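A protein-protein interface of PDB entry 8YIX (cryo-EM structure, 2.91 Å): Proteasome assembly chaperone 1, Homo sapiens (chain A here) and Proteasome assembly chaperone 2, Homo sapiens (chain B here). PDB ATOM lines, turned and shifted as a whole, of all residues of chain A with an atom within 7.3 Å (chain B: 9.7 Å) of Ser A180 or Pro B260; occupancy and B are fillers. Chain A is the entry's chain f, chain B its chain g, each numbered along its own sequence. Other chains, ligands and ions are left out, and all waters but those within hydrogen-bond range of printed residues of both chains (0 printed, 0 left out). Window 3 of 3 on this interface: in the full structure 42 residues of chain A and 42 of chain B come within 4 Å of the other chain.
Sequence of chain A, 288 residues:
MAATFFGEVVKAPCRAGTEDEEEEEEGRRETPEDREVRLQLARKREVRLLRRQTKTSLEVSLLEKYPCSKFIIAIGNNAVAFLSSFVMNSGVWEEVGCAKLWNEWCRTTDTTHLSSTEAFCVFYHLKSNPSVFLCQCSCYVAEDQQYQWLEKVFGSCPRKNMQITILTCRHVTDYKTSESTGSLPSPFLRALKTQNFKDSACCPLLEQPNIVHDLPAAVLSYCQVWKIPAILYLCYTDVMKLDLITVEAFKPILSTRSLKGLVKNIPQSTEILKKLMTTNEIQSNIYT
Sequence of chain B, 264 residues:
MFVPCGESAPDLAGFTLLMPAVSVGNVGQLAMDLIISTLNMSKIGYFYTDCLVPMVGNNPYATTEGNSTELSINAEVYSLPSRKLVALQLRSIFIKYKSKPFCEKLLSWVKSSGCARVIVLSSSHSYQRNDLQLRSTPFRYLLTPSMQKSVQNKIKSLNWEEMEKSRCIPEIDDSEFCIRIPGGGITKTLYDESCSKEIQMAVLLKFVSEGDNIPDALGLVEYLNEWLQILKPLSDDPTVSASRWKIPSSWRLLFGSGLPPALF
Among the printed residues, merely in contact across the chains: Ser A178 with Gly B258 (3.3 Å), Ser A180 with Pro B260 (3.5 Å), Ser A178 with Leu B253 (3.7 Å), Thr A177 with Leu B253 (3.7 Å), Thr A181 with Ser B257 (3.7 Å) and Ser A180 with Leu B259 (3.9 Å).
The backbone carbonyl oxygen (O) of Thr A177 sits at hydrogen-bond distance from the side-chain hydroxyl (OG) of Ser B257 (2.4 Å). The backbone carbonyl oxygen (O) of Glu A179 lies within hydrogen-bond range of the side-chain hydroxyl (OG) of Ser B257, at 3.0 Å. N of Gly B258 sits at hydrogen-bond distance from O of Thr A177. N of Gly B258 sits at hydrogen-bond distance from O of Glu A179 (2.8 Å).
The backbone carbonyl oxygen of Ser A180 is in hydrogen-bond range of the side-chain hydroxyl of Ser A183 (2.9 Å).
Printed residues of chain B within 4 Å of Ser A178: Leu B253 and Gly B258. Of the printed residues of chain B, Glu A179 touches Ser B257 (3.0 Å) and Gly B258 (2.8 Å). Ser A180 touches two residues of chain B. Thr A181 touches just one residue of chain B: Ser B257 (3.7 Å). Gly A182 touches none of the printed residues of chain B. Leu A184 touches none of the printed residues of chain B. Of the printed residues of chain A, Leu B253 touches Thr A177 (3.7 Å) and Ser A178 (3.7 Å). Printed residues of chain A within 4 Å of Ser B257: Thr A177, Glu A179 and Thr A181. Printed residues of chain A within 4 Å of Pro B260: Ser A180 (3.5 Å). Leu B263 touches none of the printed residues of chain A. The nearest residue of chain A that does not touch Pro B260 is Thr A181 (6.5 Å). The nearest printed residue of chain A that does not touch Ser B257 is Tyr A175 (4.2 Å).
Printed residues of chain B that touch a printed residue of chain A: Leu B253, Ser B257, Gly B258, Leu B259 and Pro B260. Among the printed residues, 10 pairs touch across the chains.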
ATOM      1  N   VAL A 172       8.496  27.466  -8.106  1.00  0.00           N
ATOM      2  CA  VAL A 172       8.505  26.390  -9.084  1.00  0.00           C
ATOM      3  C   VAL A 172       7.120  25.789  -9.242  1.00  0.00           C
ATOM      4  O   VAL A 172       6.809  25.204 -10.279  1.00  0.00           O
ATOM      5  CB  VAL A 172       9.547  25.333  -8.690  1.00  0.00           C
ATOM      6  CG1 VAL A 172       9.142  24.643  -7.426  1.00  0.00           C
ATOM      7  CG2 VAL A 172       9.746  24.351  -9.805  1.00  0.00           C
ATOM      8  N   TYR A 175       5.273  26.817 -12.302  1.00  0.00           N
ATOM      9  CA  TYR A 175       5.625  26.256 -13.589  1.00  0.00           C
ATOM     10  C   TYR A 175       4.570  25.250 -14.006  1.00  0.00           C
ATOM     11  O   TYR A 175       4.172  24.394 -13.217  1.00  0.00           O
ATOM     12  CB  TYR A 175       6.993  25.601 -13.517  1.00  0.00           C
ATOM     13  CG  TYR A 175       7.699  25.526 -14.834  1.00  0.00           C
ATOM     14  CD1 TYR A 175       8.085  26.660 -15.493  1.00  0.00           C
ATOM     15  CD2 TYR A 175       7.972  24.317 -15.415  1.00  0.00           C
ATOM     16  CE1 TYR A 175       8.725  26.590 -16.685  1.00  0.00           C
ATOM     17  CE2 TYR A 175       8.611  24.237 -16.605  1.00  0.00           C
ATOM     18  CZ  TYR A 175       8.983  25.373 -17.240  1.00  0.00           C
ATOM     19  OH  TYR A 175       9.631  25.291 -18.441  1.00  0.00           O
ATOM     20  N   THR A 177       4.012  22.208 -16.206  1.00  0.00           N
ATOM     21  CA  THR A 177       4.779  21.159 -16.850  1.00  0.00           C
ATOM     22  C   THR A 177       3.991  19.865 -16.766  1.00  0.00           C
ATOM     23  O   THR A 177       3.158  19.698 -15.877  1.00  0.00           O
ATOM     24  CB  THR A 177       6.154  21.018 -16.194  1.00  0.00           C
ATOM     25  OG1 THR A 177       6.920  20.022 -16.876  1.00  0.00           O
ATOM     26  CG2 THR A 177       6.023  20.670 -14.743  1.00  0.00           C
ATOM     27  N   SER A 178       4.229  18.960 -17.713  1.00  0.00           N
ATOM     28  CA  SER A 178       3.507  17.696 -17.697  1.00  0.00           C
ATOM     29  C   SER A 178       4.008  16.763 -16.610  1.00  0.00           C
ATOM     30  O   SER A 178       3.273  15.865 -16.195  1.00  0.00           O
ATOM     31  CB  SER A 178       3.591  17.009 -19.055  1.00  0.00           C
ATOM     32  OG  SER A 178       4.920  16.672 -19.376  1.00  0.00           O
ATOM     33  N   GLU A 179       5.234  16.955 -16.141  1.00  0.00           N
ATOM     34  CA  GLU A 179       5.775  16.215 -15.013  1.00  0.00           C
ATOM     35  C   GLU A 179       5.251  16.833 -13.725  1.00  0.00           C
ATOM     36  O   GLU A 179       4.390  17.710 -13.738  1.00  0.00           O
ATOM     37  CB  GLU A 179       7.295  16.221 -15.068  1.00  0.00           C
ATOM     38  CG  GLU A 179       7.852  16.069 -16.459  1.00  0.00           C
ATOM     39  CD  GLU A 179       9.367  16.064 -16.488  1.00  0.00           C
ATOM     40  OE1 GLU A 179       9.944  15.640 -17.511  1.00  0.00           O
ATOM     41  OE2 GLU A 179       9.988  16.480 -15.487  1.00  0.00           O
ATOM     42  N   SER A 180       5.765  16.394 -12.590  1.00  0.00           N
ATOM     43  CA  SER A 180       5.424  17.002 -11.316  1.00  0.00           C
ATOM     44  C   SER A 180       6.328  18.196 -11.057  1.00  0.00           C
ATOM     45  O   SER A 180       7.514  18.160 -11.377  1.00  0.00           O
ATOM     46  CB  SER A 180       5.570  15.984 -10.191  1.00  0.00           C
ATOM     47  OG  SER A 180       5.123  16.526  -8.967  1.00  0.00           O
ATOM     48  N   THR A 181       5.777  19.252 -10.461  1.00  0.00           N
ATOM     49  CA  THR A 181       6.607  20.402 -10.122  1.00  0.00           C
ATOM     50  C   THR A 181       7.339  20.146  -8.818  1.00  0.00           C
ATOM     51  O   THR A 181       7.358  21.005  -7.933  1.00  0.00           O
ATOM     52  CB  THR A 181       5.775  21.675  -9.977  1.00  0.00           C
ATOM     53  OG1 THR A 181       4.641  21.410  -9.146  1.00  0.00           O
ATOM     54  CG2 THR A 181       5.305  22.177 -11.320  1.00  0.00           C
ATOM     55  N   GLY A 182       7.924  18.963  -8.689  1.00  0.00           N
ATOM     56  CA  GLY A 182       8.760  18.621  -7.565  1.00  0.00           C
ATOM     57  C   GLY A 182       9.895  17.775  -8.071  1.00  0.00           C
ATOM     58  O   GLY A 182      10.840  17.467  -7.345  1.00  0.00           O
ATOM     59  N   SER A 183       9.799  17.398  -9.340  1.00  0.00           N
ATOM     60  CA  SER A 183      10.838  16.655 -10.028  1.00  0.00           C
ATOM     61  C   SER A 183      11.734  17.555 -10.856  1.00  0.00           C
ATOM     62  O   SER A 183      12.765  17.095 -11.351  1.00  0.00           O
ATOM     63  CB  SER A 183      10.215  15.593 -10.933  1.00  0.00           C
ATOM     64  OG  SER A 183       9.551  16.184 -12.026  1.00  0.00           O
ATOM     65  N   LEU A 184      11.363  18.811 -11.012  1.00  0.00           N
ATOM     66  CA  LEU A 184      12.161  19.742 -11.778  1.00  0.00           C
ATOM     67  C   LEU A 184      13.363  20.197 -10.958  1.00  0.00           C
ATOM     68  O   LEU A 184      13.280  20.283  -9.731  1.00  0.00           O
ATOM     69  CB  LEU A 184      11.310  20.937 -12.190  1.00  0.00           C
ATOM     70  CG  LEU A 184      10.436  20.807 -13.432  1.00  0.00           C
ATOM     71  CD1 LEU A 184       9.323  19.851 -13.241  1.00  0.00           C
ATOM     72  CD2 LEU A 184       9.867  22.150 -13.717  1.00  0.00           C
ATOM     73  N   LEU B 253      -2.046  21.346 -20.711  1.00  0.00           N
ATOM     74  CA  LEU B 253      -1.986  21.367 -19.252  1.00  0.00           C
ATOM     75  C   LEU B 253      -3.031  22.302 -18.671  1.00  0.00           C
ATOM     76  O   LEU B 253      -2.739  23.160 -17.840  1.00  0.00           O
ATOM     77  CB  LEU B 253      -0.600  21.757 -18.768  1.00  0.00           C
ATOM     78  CG  LEU B 253       0.569  21.040 -19.394  1.00  0.00           C
ATOM     79  CD1 LEU B 253       1.781  21.820 -19.079  1.00  0.00           C
ATOM     80  CD2 LEU B 253       0.655  19.695 -18.791  1.00  0.00           C
ATOM     81  N   GLY B 256      -3.573  22.203 -14.907  1.00  0.00           N
ATOM     82  CA  GLY B 256      -2.439  22.465 -14.057  1.00  0.00           C
ATOM     83  C   GLY B 256      -1.174  21.767 -14.485  1.00  0.00           C
ATOM     84  O   GLY B 256      -0.675  22.005 -15.580  1.00  0.00           O
ATOM     85  N   SER B 257      -0.635  20.915 -13.623  1.00  0.00           N
ATOM     86  CA  SER B 257       0.621  20.234 -13.897  1.00  0.00           C
ATOM     87  C   SER B 257       0.487  18.748 -13.615  1.00  0.00           C
ATOM     88  O   SER B 257      -0.624  18.249 -13.452  1.00  0.00           O
ATOM     89  CB  SER B 257       1.747  20.829 -13.069  1.00  0.00           C
ATOM     90  OG  SER B 257       2.988  20.369 -13.548  1.00  0.00           O
ATOM     91  N   GLY B 258       1.595  18.037 -13.555  1.00  0.00           N
ATOM     92  CA  GLY B 258       1.544  16.596 -13.437  1.00  0.00           C
ATOM     93  C   GLY B 258       1.278  16.101 -12.037  1.00  0.00           C
ATOM     94  O   GLY B 258       1.332  16.835 -11.060  1.00  0.00           O
ATOM     95  N   LEU B 259       1.026  14.813 -11.950  1.00  0.00           N
ATOM     96  CA  LEU B 259       0.614  14.174 -10.706  1.00  0.00           C
ATOM     97  C   LEU B 259       1.823  13.906  -9.815  1.00  0.00           C
ATOM     98  O   LEU B 259       2.790  13.293 -10.267  1.00  0.00           O
ATOM     99  CB  LEU B 259      -0.114  12.876 -11.020  1.00  0.00           C
ATOM    100  CG  LEU B 259      -0.647  11.995  -9.902  1.00  0.00           C
ATOM    101  CD1 LEU B 259      -1.815  12.630  -9.227  1.00  0.00           C
ATOM    102  CD2 LEU B 259      -1.029  10.657 -10.450  1.00  0.00           C
ATOM    103  N   PRO B 260       1.803  14.340  -8.555  1.00  0.00           N
ATOM    104  CA  PRO B 260       2.936  14.075  -7.679  1.00  0.00           C
ATOM    105  C   PRO B 260       3.074  12.591  -7.402  1.00  0.00           C
ATOM    106  O   PRO B 260       2.080  11.848  -7.415  1.00  0.00           O
ATOM    107  CB  PRO B 260       2.577  14.846  -6.397  1.00  0.00           C
ATOM    108  CG  PRO B 260       1.570  15.804  -6.801  1.00  0.00           C
ATOM    109  CD  PRO B 260       0.791  15.161  -7.884  1.00  0.00           C
ATOM    110  N   PRO B 261       4.282  12.113  -7.147  1.00  0.00           N
ATOM    111  CA  PRO B 261       4.467  10.708  -6.792  1.00  0.00           C
ATOM    112  C   PRO B 261       4.079  10.447  -5.343  1.00  0.00           C
ATOM    113  O   PRO B 261       3.836  11.361  -4.559  1.00  0.00           O
ATOM    114  CB  PRO B 261       5.961  10.500  -7.015  1.00  0.00           C
ATOM    115  CG  PRO B 261       6.532  11.804  -6.686  1.00  0.00           C
ATOM    116  CD  PRO B 261       5.569  12.819  -7.214  1.00  0.00           C
ATOM    117  N   ALA B 262       3.989   9.157  -5.015  1.00  0.00           N
ATOM    118  CA  ALA B 262       3.722   8.645  -3.674  1.00  0.00           C
ATOM    119  C   ALA B 262       2.281   8.881  -3.243  1.00  0.00           C
ATOM    120  O   ALA B 262       1.858   8.383  -2.202  1.00  0.00           O
ATOM    121  CB  ALA B 262       4.681   9.241  -2.649  1.00  0.00           C
ATOM    122  N   LEU B 263       1.526   9.637  -4.030  1.00  0.00           N
ATOM    123  CA  LEU B 263       0.077   9.559  -4.022  1.00  0.00           C
ATOM    124  C   LEU B 263      -0.296   8.542  -5.082  1.00  0.00           C
ATOM    125  O   LEU B 263       0.362   8.464  -6.124  1.00  0.00           O
ATOM    126  CB  LEU B 263      -0.557  10.906  -4.359  1.00  0.00           C
ATOM    127  CG  LEU B 263      -0.288  12.129  -3.502  1.00  0.00           C
ATOM    128  CD1 LEU B 263      -0.463  13.334  -4.349  1.00  0.00           C
ATOM    129  CD2 LEU B 263      -1.269  12.175  -2.393  1.00  0.00           C
ATOM    130  N   PHE B 264      -1.332   7.755  -4.819  1.00  0.00           N
ATOM    131  CA  PHE B 264      -1.748   6.713  -5.756  1.00  0.00           C
ATOM    132  C   PHE B 264      -0.645   5.675  -5.926  1.00  0.00           C
ATOM    133  O   PHE B 264      -0.789   4.708  -6.667  1.00  0.00           O
ATOM    134  CB  PHE B 264      -2.129   7.304  -7.115  1.00  0.00           C
ATOM    135  CG  PHE B 264      -3.170   8.365  -7.037  1.00  0.00           C
ATOM    136  CD1 PHE B 264      -4.495   8.042  -6.935  1.00  0.00           C
ATOM    137  CD2 PHE B 264      -2.824   9.690  -7.067  1.00  0.00           C
ATOM    138  CE1 PHE B 264      -5.442   9.019  -6.849  1.00  0.00           C
ATOM    139  CE2 PHE B 264      -3.773  10.662  -6.991  1.00  0.00           C
ATOM    140  CZ  PHE B 264      -5.079  10.325  -6.881  1.00  0.00           C
ATOM    141  OXT PHE B 264       0.423   5.751  -5.329  1.00  0.00           O
